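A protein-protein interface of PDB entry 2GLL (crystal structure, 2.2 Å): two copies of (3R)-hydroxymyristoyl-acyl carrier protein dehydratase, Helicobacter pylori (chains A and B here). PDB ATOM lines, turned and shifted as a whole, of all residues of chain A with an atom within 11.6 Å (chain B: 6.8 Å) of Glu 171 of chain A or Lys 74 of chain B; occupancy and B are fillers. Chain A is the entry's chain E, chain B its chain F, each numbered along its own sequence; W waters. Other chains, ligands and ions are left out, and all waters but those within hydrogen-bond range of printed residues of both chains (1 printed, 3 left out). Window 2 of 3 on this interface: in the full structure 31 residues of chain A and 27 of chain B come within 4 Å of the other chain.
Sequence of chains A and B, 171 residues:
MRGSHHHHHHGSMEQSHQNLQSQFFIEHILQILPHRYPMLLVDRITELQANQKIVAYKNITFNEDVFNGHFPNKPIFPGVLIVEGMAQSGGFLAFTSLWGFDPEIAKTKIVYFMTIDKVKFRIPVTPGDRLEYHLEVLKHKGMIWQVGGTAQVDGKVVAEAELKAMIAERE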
ATOM      1  N   PRO A  34      -7.718  19.250  -5.524  1.00  0.00           N
ATOM      2  CA  PRO A  34      -6.994  18.987  -4.282  1.00  0.00           C
ATOM      3  C   PRO A  34      -7.568  17.803  -3.513  1.00  0.00           C
ATOM      4  O   PRO A  34      -6.856  17.145  -2.761  1.00  0.00           O
ATOM      5  CB  PRO A  34      -7.141  20.306  -3.523  1.00  0.00           C
ATOM      6  CG  PRO A  34      -8.511  20.741  -3.906  1.00  0.00           C
ATOM      7  CD  PRO A  34      -8.554  20.458  -5.402  1.00  0.00           C
ATOM      8  N   HIS A  35      -8.852  17.535  -3.722  1.00  0.00           N
ATOM      9  CA  HIS A  35      -9.547  16.451  -3.040  1.00  0.00           C
ATOM     10  C   HIS A  35      -8.851  15.105  -3.165  1.00  0.00           C
ATOM     11  O   HIS A  35      -8.298  14.773  -4.214  1.00  0.00           O
ATOM     12  CB  HIS A  35     -10.965  16.308  -3.579  1.00  0.00           C
ATOM     13  CG  HIS A  35     -11.739  17.585  -3.594  1.00  0.00           C
ATOM     14  ND1 HIS A  35     -11.431  18.631  -4.437  1.00  0.00           N
ATOM     15  CD2 HIS A  35     -12.809  17.986  -2.870  1.00  0.00           C
ATOM     16  CE1 HIS A  35     -12.279  19.622  -4.230  1.00  0.00           C
ATOM     17  NE2 HIS A  35     -13.125  19.256  -3.283  1.00  0.00           N
ATOM     18  N   ARG A  36      -8.891  14.328  -2.085  1.00  0.00           N
ATOM     19  CA  ARG A  36      -8.284  13.011  -2.066  1.00  0.00           C
ATOM     20  C   ARG A  36      -9.218  12.020  -1.395  1.00  0.00           C
ATOM     21  O   ARG A  36     -10.254  12.410  -0.866  1.00  0.00           O
ATOM     22  CB  ARG A  36      -6.937  13.066  -1.354  1.00  0.00           C
ATOM     23  CG  ARG A  36      -5.832  13.650  -2.223  1.00  0.00           C
ATOM     24  CD  ARG A  36      -5.643  12.797  -3.468  1.00  0.00           C
ATOM     25  NE  ARG A  36      -4.549  13.256  -4.315  1.00  0.00           N
ATOM     26  CZ  ARG A  36      -4.601  14.314  -5.120  1.00  0.00           C
ATOM     27  NH1 ARG A  36      -3.540  14.638  -5.843  1.00  0.00           N
ATOM     28  NH2 ARG A  36      -5.709  15.041  -5.219  1.00  0.00           N
ATOM     29  N   TYR A  37      -8.872  10.736  -1.429  1.00  0.00           N
ATOM     30  CA  TYR A  37      -9.730   9.718  -0.826  1.00  0.00           C
ATOM     31  C   TYR A  37      -9.962  10.020   0.647  1.00  0.00           C
ATOM     32  O   TYR A  37      -9.042  10.409   1.349  1.00  0.00           O
ATOM     33  CB  TYR A  37      -9.108   8.325  -0.984  1.00  0.00           C
ATOM     34  CG  TYR A  37      -9.928   7.216  -0.359  1.00  0.00           C
ATOM     35  CD1 TYR A  37      -9.810   6.913   1.001  1.00  0.00           C
ATOM     36  CD2 TYR A  37     -10.835   6.475  -1.123  1.00  0.00           C
ATOM     37  CE1 TYR A  37     -10.566   5.907   1.581  1.00  0.00           C
ATOM     38  CE2 TYR A  37     -11.599   5.460  -0.551  1.00  0.00           C
ATOM     39  CZ  TYR A  37     -11.457   5.181   0.801  1.00  0.00           C
ATOM     40  OH  TYR A  37     -12.188   4.168   1.369  1.00  0.00           O
ATOM     41  N   MET A  39     -12.721  11.575  -0.441  1.00  0.00           N
ATOM     42  CA  MET A  39     -13.509  12.748  -0.776  1.00  0.00           C
ATOM     43  C   MET A  39     -13.319  13.276  -2.206  1.00  0.00           C
ATOM     44  O   MET A  39     -13.675  14.417  -2.511  1.00  0.00           O
ATOM     45  CB  MET A  39     -13.214  13.839   0.250  1.00  0.00           C
ATOM     46  CG  MET A  39     -14.415  14.680   0.650  1.00  0.00           C
ATOM     47  SD  MET A  39     -15.845  13.749   1.282  1.00  0.00           S
ATOM     48  CE  MET A  39     -17.120  14.641   0.511  1.00  0.00           C
ATOM     49  N   ILE A 105       0.723  24.655 -10.290  1.00  0.00           N
ATOM     50  CA  ILE A 105      -0.033  25.780  -9.749  1.00  0.00           C
ATOM     51  C   ILE A 105      -1.195  25.242  -8.919  1.00  0.00           C
ATOM     52  O   ILE A 105      -1.531  25.785  -7.867  1.00  0.00           O
ATOM     53  CB  ILE A 105      -0.633  26.654 -10.868  1.00  0.00           C
ATOM     54  CG1 ILE A 105       0.461  27.474 -11.552  1.00  0.00           C
ATOM     55  CG2 ILE A 105      -1.726  27.539 -10.296  1.00  0.00           C
ATOM     56  CD1 ILE A 105      -0.043  28.303 -12.721  1.00  0.00           C
ATOM     57  N   ALA A 106      -1.807  24.166  -9.403  1.00  0.00           N
ATOM     58  CA  ALA A 106      -2.954  23.576  -8.724  1.00  0.00           C
ATOM     59  C   ALA A 106      -2.656  22.856  -7.408  1.00  0.00           C
ATOM     60  O   ALA A 106      -3.530  22.776  -6.544  1.00  0.00           O
ATOM     61  CB  ALA A 106      -3.680  22.619  -9.678  1.00  0.00           C
ATOM     62  N   LYS A 107      -1.440  22.346  -7.236  1.00  0.00           N
ATOM     63  CA  LYS A 107      -1.139  21.610  -6.016  1.00  0.00           C
ATOM     64  C   LYS A 107      -1.243  22.388  -4.699  1.00  0.00           C
ATOM     65  O   LYS A 107      -1.370  21.773  -3.639  1.00  0.00           O
ATOM     66  CB  LYS A 107       0.226  20.917  -6.124  1.00  0.00           C
ATOM     67  CG  LYS A 107       1.435  21.807  -5.973  1.00  0.00           C
ATOM     68  CD  LYS A 107       2.711  21.006  -6.205  1.00  0.00           C
ATOM     69  CE  LYS A 107       3.919  21.656  -5.519  1.00  0.00           C
ATOM     70  NZ  LYS A 107       3.835  21.638  -4.008  1.00  0.00           N
ATOM     71  N   THR A 108      -1.217  23.720  -4.751  1.00  0.00           N
ATOM     72  CA  THR A 108      -1.320  24.520  -3.529  1.00  0.00           C
ATOM     73  C   THR A 108      -2.657  25.241  -3.412  1.00  0.00           C
ATOM     74  O   THR A 108      -2.815  26.143  -2.586  1.00  0.00           O
ATOM     75  CB  THR A 108      -0.187  25.580  -3.424  1.00  0.00           C
ATOM     76  OG1 THR A 108      -0.155  26.377  -4.616  1.00  0.00           O
ATOM     77  CG2 THR A 108       1.161  24.906  -3.224  1.00  0.00           C
ATOM     78  N   LYS A 109      -3.619  24.841  -4.238  1.00  0.00           N
ATOM     79  CA  LYS A 109      -4.941  25.459  -4.207  1.00  0.00           C
ATOM     80  C   LYS A 109      -5.952  24.588  -3.464  1.00  0.00           C
ATOM     81  O   LYS A 109      -5.834  23.360  -3.419  1.00  0.00           O
ATOM     82  CB  LYS A 109      -5.468  25.690  -5.626  1.00  0.00           C
ATOM     83  CG  LYS A 109      -4.535  26.409  -6.568  1.00  0.00           C
ATOM     84  CD  LYS A 109      -4.391  27.874  -6.223  1.00  0.00           C
ATOM     85  CE  LYS A 109      -3.627  28.591  -7.319  1.00  0.00           C
ATOM     86  NZ  LYS A 109      -3.279  29.981  -6.935  1.00  0.00           N
ATOM     87  N   ILE A 110      -6.951  25.242  -2.890  1.00  0.00           N
ATOM     88  CA  ILE A 110      -8.016  24.553  -2.187  1.00  0.00           C
ATOM     89  C   ILE A 110      -9.321  25.105  -2.755  1.00  0.00           C
ATOM     90  O   ILE A 110      -9.309  26.091  -3.506  1.00  0.00           O
ATOM     91  CB  ILE A 110      -7.929  24.791  -0.660  1.00  0.00           C
ATOM     92  CG1 ILE A 110      -6.730  24.025  -0.100  1.00  0.00           C
ATOM     93  CG2 ILE A 110      -9.200  24.308   0.036  1.00  0.00           C
ATOM     94  CD1 ILE A 110      -6.787  23.793   1.396  1.00  0.00           C
ATOM     95  N   VAL A 111     -10.433  24.455  -2.427  1.00  0.00           N
ATOM     96  CA  VAL A 111     -11.748  24.882  -2.901  1.00  0.00           C
ATOM     97  C   VAL A 111     -12.763  24.953  -1.759  1.00  0.00           C
ATOM     98  O   VAL A 111     -13.037  23.949  -1.096  1.00  0.00           O
ATOM     99  CB  VAL A 111     -12.299  23.910  -3.961  1.00  0.00           C
ATOM    100  CG1 VAL A 111     -13.735  24.270  -4.293  1.00  0.00           C
ATOM    101  CG2 VAL A 111     -11.436  23.961  -5.209  1.00  0.00           C
ATOM    102  N   TYR A 112     -13.316  26.142  -1.534  1.00  0.00           N
ATOM    103  CA  TYR A 112     -14.307  26.342  -0.481  1.00  0.00           C
ATOM    104  C   TYR A 112     -15.689  26.508  -1.086  1.00  0.00           C
ATOM    105  O   TYR A 112     -15.863  27.189  -2.102  1.00  0.00           O
ATOM    106  CB  TYR A 112     -14.026  27.612   0.341  1.00  0.00           C
ATOM    107  CG  TYR A 112     -12.791  27.587   1.207  1.00  0.00           C
ATOM    108  CD1 TYR A 112     -11.566  28.021   0.716  1.00  0.00           C
ATOM    109  CD2 TYR A 112     -12.853  27.134   2.527  1.00  0.00           C
ATOM    110  CE1 TYR A 112     -10.426  28.006   1.520  1.00  0.00           C
ATOM    111  CE2 TYR A 112     -11.722  27.115   3.340  1.00  0.00           C
ATOM    112  CZ  TYR A 112     -10.510  27.552   2.831  1.00  0.00           C
ATOM    113  OH  TYR A 112      -9.379  27.541   3.629  1.00  0.00           O
ATOM    114  N   PHE A 113     -16.670  25.883  -0.448  1.00  0.00           N
ATOM    115  CA  PHE A 113     -18.054  25.998  -0.867  1.00  0.00           C
ATOM    116  C   PHE A 113     -18.492  27.351  -0.318  1.00  0.00           C
ATOM    117  O   PHE A 113     -18.103  27.717   0.785  1.00  0.00           O
ATOM    118  CB  PHE A 113     -18.885  24.901  -0.203  1.00  0.00           C
ATOM    119  CG  PHE A 113     -19.528  23.960  -1.163  1.00  0.00           C
ATOM    120  CD1 PHE A 113     -20.539  24.399  -2.012  1.00  0.00           C
ATOM    121  CD2 PHE A 113     -19.122  22.630  -1.224  1.00  0.00           C
ATOM    122  CE1 PHE A 113     -21.144  23.517  -2.915  1.00  0.00           C
ATOM    123  CE2 PHE A 113     -19.718  21.744  -2.120  1.00  0.00           C
ATOM    124  CZ  PHE A 113     -20.732  22.191  -2.967  1.00  0.00           C
ATOM    125  N   MET A 143     -11.773  34.271  -8.581  1.00  0.00           N
ATOM    126  CA  MET A 143     -11.788  32.938  -7.984  1.00  0.00           C
ATOM    127  C   MET A 143     -13.188  32.425  -7.663  1.00  0.00           C
ATOM    128  O   MET A 143     -13.344  31.274  -7.253  1.00  0.00           O
ATOM    129  CB  MET A 143     -10.981  32.939  -6.681  1.00  0.00           C
ATOM    130  CG  MET A 143      -9.550  33.393  -6.816  1.00  0.00           C
ATOM    131  SD  MET A 143      -8.623  32.301  -7.906  1.00  0.00           S
ATOM    132  CE  MET A 143      -8.618  33.295  -9.398  1.00  0.00           C
ATOM    133  N   MET A 166     -15.322  28.819  -4.263  1.00  0.00           N
ATOM    134  CA  MET A 166     -14.173  29.702  -4.378  1.00  0.00           C
ATOM    135  C   MET A 166     -12.841  28.976  -4.392  1.00  0.00           C
ATOM    136  O   MET A 166     -12.575  28.147  -3.527  1.00  0.00           O
ATOM    137  CB  MET A 166     -14.167  30.698  -3.217  1.00  0.00           C
ATOM    138  CG  MET A 166     -12.903  31.533  -3.106  1.00  0.00           C
ATOM    139  SD  MET A 166     -13.055  32.735  -1.764  1.00  0.00           S
ATOM    140  CE  MET A 166     -13.969  34.024  -2.589  1.00  0.00           C
ATOM    141  N   ILE A 167     -12.005  29.297  -5.374  1.00  0.00           N
ATOM    142  CA  ILE A 167     -10.681  28.706  -5.448  1.00  0.00           C
ATOM    143  C   ILE A 167      -9.773  29.620  -4.633  1.00  0.00           C
ATOM    144  O   ILE A 167      -9.800  30.830  -4.807  1.00  0.00           O
ATOM    145  CB  ILE A 167     -10.136  28.650  -6.887  1.00  0.00           C
ATOM    146  CG1 ILE A 167     -10.973  27.691  -7.731  1.00  0.00           C
ATOM    147  CG2 ILE A 167      -8.672  28.193  -6.860  1.00  0.00           C
ATOM    148  CD1 ILE A 167     -10.446  27.511  -9.151  1.00  0.00           C
ATOM    149  N   ALA A 168      -8.978  29.043  -3.741  1.00  0.00           N
ATOM    150  CA  ALA A 168      -8.090  29.843  -2.914  1.00  0.00           C
ATOM    151  C   ALA A 168      -6.708  29.226  -2.741  1.00  0.00           C
ATOM    152  O   ALA A 168      -6.565  28.005  -2.690  1.00  0.00           O
ATOM    153  CB  ALA A 168      -8.721  30.064  -1.558  1.00  0.00           C
ATOM    154  N   GLU A 169      -5.691  30.081  -2.664  1.00  0.00           N
ATOM    155  CA  GLU A 169      -4.324  29.625  -2.456  1.00  0.00           C
ATOM    156  C   GLU A 169      -4.271  29.152  -1.007  1.00  0.00           C
ATOM    157  O   GLU A 169      -4.756  29.829  -0.099  1.00  0.00           O
ATOM    158  CB  GLU A 169      -3.329  30.776  -2.668  1.00  0.00           C
ATOM    159  CG  GLU A 169      -1.841  30.408  -2.487  1.00  0.00           C
ATOM    160  CD  GLU A 169      -1.356  29.396  -3.512  1.00  0.00           C
ATOM    161  OE1 GLU A 169      -1.929  29.362  -4.614  1.00  0.00           O
ATOM    162  OE2 GLU A 169      -0.402  28.647  -3.234  1.00  0.00           O
ATOM    163  N   ARG A 170      -3.693  27.979  -0.795  1.00  0.00           N
ATOM    164  CA  ARG A 170      -3.582  27.412   0.540  1.00  0.00           C
ATOM    165  C   ARG A 170      -2.586  28.186   1.403  1.00  0.00           C
ATOM    166  O   ARG A 170      -1.463  28.461   0.982  1.00  0.00           O
ATOM    167  CB  ARG A 170      -3.133  25.952   0.428  1.00  0.00           C
ATOM    168  CG  ARG A 170      -3.131  25.153   1.713  1.00  0.00           C
ATOM    169  CD  ARG A 170      -2.667  23.734   1.393  1.00  0.00           C
ATOM    170  NE  ARG A 170      -3.409  23.214   0.247  1.00  0.00           N
ATOM    171  CZ  ARG A 170      -3.017  22.197  -0.522  1.00  0.00           C
ATOM    172  NH1 ARG A 170      -1.869  21.567  -0.270  1.00  0.00           N
ATOM    173  NH2 ARG A 170      -3.771  21.820  -1.561  1.00  0.00           N
ATOM    174  N   GLU A 171      -3.006  28.562   2.605  1.00  0.00           N
ATOM    175  CA  GLU A 171      -2.102  29.253   3.513  1.00  0.00           C
ATOM    176  C   GLU A 171      -2.284  28.712   4.920  1.00  0.00           C
ATOM    177  O   GLU A 171      -3.149  27.821   5.092  1.00  0.00           O
ATOM    178  CB  GLU A 171      -2.311  30.773   3.468  1.00  0.00           C
ATOM    179  CG  GLU A 171      -3.743  31.258   3.530  1.00  0.00           C
ATOM    180  CD  GLU A 171      -3.833  32.783   3.410  1.00  0.00           C
ATOM    181  OE1 GLU A 171      -3.217  33.479   4.252  1.00  0.00           O
ATOM    182  OE2 GLU A 171      -4.511  33.288   2.486  1.00  0.00           O
ATOM    183  OXT GLU A 171      -1.541  29.157   5.826  1.00  0.00           O
ATOM    184  N   PHE B  67     -11.146  13.578   6.747  1.00  0.00           N
ATOM    185  CA  PHE B  67     -10.044  14.537   6.676  1.00  0.00           C
ATOM    186  C   PHE B  67      -8.822  14.072   5.879  1.00  0.00           C
ATOM    187  O   PHE B  67      -7.994  14.887   5.482  1.00  0.00           O
ATOM    188  CB  PHE B  67      -9.636  14.984   8.083  1.00  0.00           C
ATOM    189  CG  PHE B  67     -10.653  15.878   8.746  1.00  0.00           C
ATOM    190  CD1 PHE B  67     -11.360  15.450   9.866  1.00  0.00           C
ATOM    191  CD2 PHE B  67     -10.935  17.138   8.219  1.00  0.00           C
ATOM    192  CE1 PHE B  67     -12.332  16.258  10.451  1.00  0.00           C
ATOM    193  CE2 PHE B  67     -11.903  17.951   8.794  1.00  0.00           C
ATOM    194  CZ  PHE B  67     -12.606  17.510   9.914  1.00  0.00           C
ATOM    195  N   HIS B  70      -9.828  15.730   2.690  1.00  0.00           N
ATOM    196  CA  HIS B  70     -10.444  17.044   2.639  1.00  0.00           C
ATOM    197  C   HIS B  70      -9.973  18.024   3.721  1.00  0.00           C
ATOM    198  O   HIS B  70     -10.695  18.267   4.681  1.00  0.00           O
ATOM    199  CB  HIS B  70     -11.964  16.865   2.710  1.00  0.00           C
ATOM    200  CG  HIS B  70     -12.737  18.108   2.403  1.00  0.00           C
ATOM    201  ND1 HIS B  70     -12.762  19.198   3.245  1.00  0.00           N
ATOM    202  CD2 HIS B  70     -13.491  18.445   1.331  1.00  0.00           C
ATOM    203  CE1 HIS B  70     -13.497  20.151   2.705  1.00  0.00           C
ATOM    204  NE2 HIS B  70     -13.951  19.720   1.543  1.00  0.00           N
ATOM    205  N   PHE B  71      -8.773  18.586   3.588  1.00  0.00           N
ATOM    206  CA  PHE B  71      -7.863  18.318   2.481  1.00  0.00           C
ATOM    207  C   PHE B  71      -6.537  17.939   3.105  1.00  0.00           C
ATOM    208  O   PHE B  71      -6.258  18.314   4.241  1.00  0.00           O
ATOM    209  CB  PHE B  71      -7.641  19.572   1.629  1.00  0.00           C
ATOM    210  CG  PHE B  71      -8.882  20.108   0.980  1.00  0.00           C
ATOM    211  CD1 PHE B  71      -9.615  21.129   1.581  1.00  0.00           C
ATOM    212  CD2 PHE B  71      -9.314  19.602  -0.248  1.00  0.00           C
ATOM    213  CE1 PHE B  71     -10.761  21.640   0.968  1.00  0.00           C
ATOM    214  CE2 PHE B  71     -10.459  20.110  -0.869  1.00  0.00           C
ATOM    215  CZ  PHE B  71     -11.182  21.131  -0.258  1.00  0.00           C
ATOM    216  N   PRO B  72      -5.702  17.173   2.386  1.00  0.00           N
ATOM    217  CA  PRO B  72      -4.426  16.842   3.026  1.00  0.00           C
ATOM    218  C   PRO B  72      -3.692  18.110   3.495  1.00  0.00           C
ATOM    219  O   PRO B  72      -3.604  19.107   2.761  1.00  0.00           O
ATOM    220  CB  PRO B  72      -3.667  16.065   1.942  1.00  0.00           C
ATOM    221  CG  PRO B  72      -4.516  16.177   0.688  1.00  0.00           C
ATOM    222  CD  PRO B  72      -5.917  16.371   1.171  1.00  0.00           C
ATOM    223  N   ASN B  73      -3.197  18.074   4.731  1.00  0.00           N
ATOM    224  CA  ASN B  73      -2.482  19.208   5.321  1.00  0.00           C
ATOM    225  C   ASN B  73      -3.365  20.404   5.665  1.00  0.00           C
ATOM    226  O   ASN B  73      -2.887  21.404   6.200  1.00  0.00           O
ATOM    227  CB  ASN B  73      -1.363  19.675   4.391  1.00  0.00           C
ATOM    228  CG  ASN B  73      -0.092  18.875   4.568  1.00  0.00           C
ATOM    229  OD1 ASN B  73      -0.039  17.674   4.260  1.00  0.00           O
ATOM    230  ND2 ASN B  73       0.944  19.531   5.082  1.00  0.00           N
ATOM    231  N   LYS B  74      -4.648  20.313   5.357  1.00  0.00           N
ATOM    232  CA  LYS B  74      -5.564  21.408   5.659  1.00  0.00           C
ATOM    233  C   LYS B  74      -6.942  20.805   5.938  1.00  0.00           C
ATOM    234  O   LYS B  74      -7.820  20.799   5.072  1.00  0.00           O
ATOM    235  CB  LYS B  74      -5.625  22.373   4.469  1.00  0.00           C
ATOM    236  CG  LYS B  74      -6.184  23.751   4.792  1.00  0.00           C
ATOM    237  CD  LYS B  74      -5.287  24.479   5.778  1.00  0.00           C
ATOM    238  CE  LYS B  74      -5.557  25.976   5.770  1.00  0.00           C
ATOM    239  NZ  LYS B  74      -7.024  26.262   5.838  1.00  0.00           N
ATOM    240  N   PRO B  75      -7.137  20.268   7.157  1.00  0.00           N
ATOM    241  CA  PRO B  75      -8.421  19.660   7.524  1.00  0.00           C
ATOM    242  C   PRO B  75      -9.569  20.645   7.640  1.00  0.00           C
ATOM    243  O   PRO B  75      -9.549  21.566   8.458  1.00  0.00           O
ATOM    244  CB  PRO B  75      -8.115  18.948   8.842  1.00  0.00           C
ATOM    245  CG  PRO B  75      -7.013  19.779   9.431  1.00  0.00           C
ATOM    246  CD  PRO B  75      -6.143  20.094   8.231  1.00  0.00           C
ATOM    247  N   ILE B  76     -10.568  20.436   6.796  1.00  0.00           N
ATOM    248  CA  ILE B  76     -11.756  21.273   6.769  1.00  0.00           C
ATOM    249  C   ILE B  76     -12.967  20.355   6.667  1.00  0.00           C
ATOM    250  O   ILE B  76     -13.074  19.566   5.725  1.00  0.00           O
ATOM    251  CB  ILE B  76     -11.695  22.235   5.567  1.00  0.00           C
ATOM    252  CG1 ILE B  76     -10.595  23.267   5.820  1.00  0.00           C
ATOM    253  CG2 ILE B  76     -13.053  22.901   5.329  1.00  0.00           C
ATOM    254  CD1 ILE B  76     -10.327  24.162   4.652  1.00  0.00           C
ATOM    255  N   PHE B  77     -13.868  20.439   7.645  1.00  0.00           N
ATOM    256  CA  PHE B  77     -15.052  19.589   7.634  1.00  0.00           C
ATOM    257  C   PHE B  77     -15.879  20.001   6.421  1.00  0.00           C
ATOM    258  O   PHE B  77     -16.216  21.173   6.269  1.00  0.00           O
ATOM    259  CB  PHE B  77     -15.861  19.770   8.925  1.00  0.00           C
ATOM    260  CG  PHE B  77     -16.862  18.668   9.180  1.00  0.00           C
ATOM    261  CD1 PHE B  77     -16.436  17.377   9.481  1.00  0.00           C
ATOM    262  CD2 PHE B  77     -18.228  18.930   9.144  1.00  0.00           C
ATOM    263  CE1 PHE B  77     -17.351  16.358   9.747  1.00  0.00           C
ATOM    264  CE2 PHE B  77     -19.160  17.923   9.407  1.00  0.00           C
ATOM    265  CZ  PHE B  77     -18.719  16.628   9.712  1.00  0.00           C
ATOM    266  N   PRO B 124     -15.167  28.275   8.132  1.00  0.00           N
ATOM    267  CA  PRO B 124     -14.807  26.859   7.989  1.00  0.00           C
ATOM    268  C   PRO B 124     -14.793  26.142   9.341  1.00  0.00           C
ATOM    269  O   PRO B 124     -14.332  26.697  10.334  1.00  0.00           O
ATOM    270  CB  PRO B 124     -13.420  26.916   7.353  1.00  0.00           C
ATOM    271  CG  PRO B 124     -12.864  28.194   7.881  1.00  0.00           C
ATOM    272  CD  PRO B 124     -14.038  29.141   7.752  1.00  0.00           C
ATOM    273  N   THR B 126     -13.452  23.075  11.672  1.00  0.00           N
ATOM    274  CA  THR B 126     -12.230  22.277  11.722  1.00  0.00           C
ATOM    275  C   THR B 126     -12.110  21.415  12.976  1.00  0.00           C
ATOM    276  O   THR B 126     -12.892  21.559  13.911  1.00  0.00           O
ATOM    277  CB  THR B 126     -10.996  23.190  11.685  1.00  0.00           C
ATOM    278  OG1 THR B 126     -10.942  23.952  12.899  1.00  0.00           O
ATOM    279  CG2 THR B 126     -11.069  24.139  10.501  1.00  0.00           C
HETATM  280  O   HOH W   1      -0.836  19.250   0.844  1.00  0.00           O
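No position is printed for both chains.
Of the 21 printed residues of chain A, 7 touch a printed residue of chain B.
Hydrophobic or aromatic side chains of chain A within 4 Å of the printed part of chain B: Pro 34, His 35, Met 39, Ile 110 and Tyr 112.
Of the 11 printed residues of chain B, 4 touch a printed residue of chain A.
Hydrophobic or aromatic side chains of chain B within 4 Å of the printed part of chain A: His 70, Phe 71 and Ile 76.
Among the printed residues, no Asp or Glu carboxylate lies within 4 Å of a Lys or Arg side-chain nitrogen of the other chain.
The backbone carbonyl oxygen (O) of Pro 34 of chain A lies within hydrogen-bond range of the guanidinium group (NH2) of Arg 36 of chain A.
O of Ala 168 of chain A lies within hydrogen-bond range of N of Ile 110 of chain A, at 2.8 Å.
The backbone carbonyl oxygen (O) of Tyr 112 of chain A lies within hydrogen-bond range of the backbone NH (N) of Met 166 of chain A.
A ring nitrogen (ND1) of His 70 of chain B is in hydrogen-bond range of the backbone carbonyl oxygen of Ile 76 of chain B.
Printed residues of chain B within 4 Å of Pro 34 of chain A: Phe 71.
Of the printed residues of chain B, His 35 of chain A touches Phe 71 (3.7 Å).
Of the printed residues of chain B, Ile 110 of chain A touches Phe 71 (3.2 Å) and Lys 74 (3.4 Å).
Of the printed residues of chain B, Val 111 of chain A touches Phe 71 (3.5 Å).
Printed residues of chain B within 4 Å of Tyr 112 of chain A: Lys 74 and Ile 76.
Of chain B, only Lys 74 comes within 4 Å of Glu 171 of chain A.
Phe 71 of chain B touches just these residues of chain A: Pro 34 (3.7 Å), His 35 (3.7 Å), Ile 110 (3.2 Å) and Val 111 (3.5 Å).
No residue of chain A comes within 4 Å of Pro 72 of chain B.
No residue of chain A comes within 4 Å of Asn 73 of chain B.
Lys 74 of chain B touches three residues of chain A.
No residue of chain A comes within 4 Å of Pro 75 of chain B.
Ile 76 of chain B touches just one residue of chain A: Tyr 112.
The nearest residue of chain B that does not touch Glu 171 of chain A is Asn 73 of chain B (6.5 Å).
The nearest residue of chain A that does not touch Lys 74 of chain B is Arg 170 of chain A (4.5 Å).
Among the printed residues, merely in contact across the chains: Glu 171 of chain A with Lys 74 of chain B, Ile 110 of chain A with Phe 71 of chain B, Ile 110 of chain A with Lys 74 of chain B, Val 111 of chain A with Phe 71 of chain B, Tyr 112 of chain A with Ile 76 of chain B, Pro 34 of chain A with Phe 71 of chain B, His 35 of chain A with Phe 71 of chain B and Met 39 of chain A with His 70 of chain B.
OH of Tyr 112 of chain A sits at hydrogen-bond distance from NZ of Lys 74 of chain B, at 3.5 Å.
Water W1 bridges the guanidinium group of Arg 170 of chain A (2.8 Å) and the backbone carbonyl oxygen of Pro 72 of chain B (3.4 Å).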
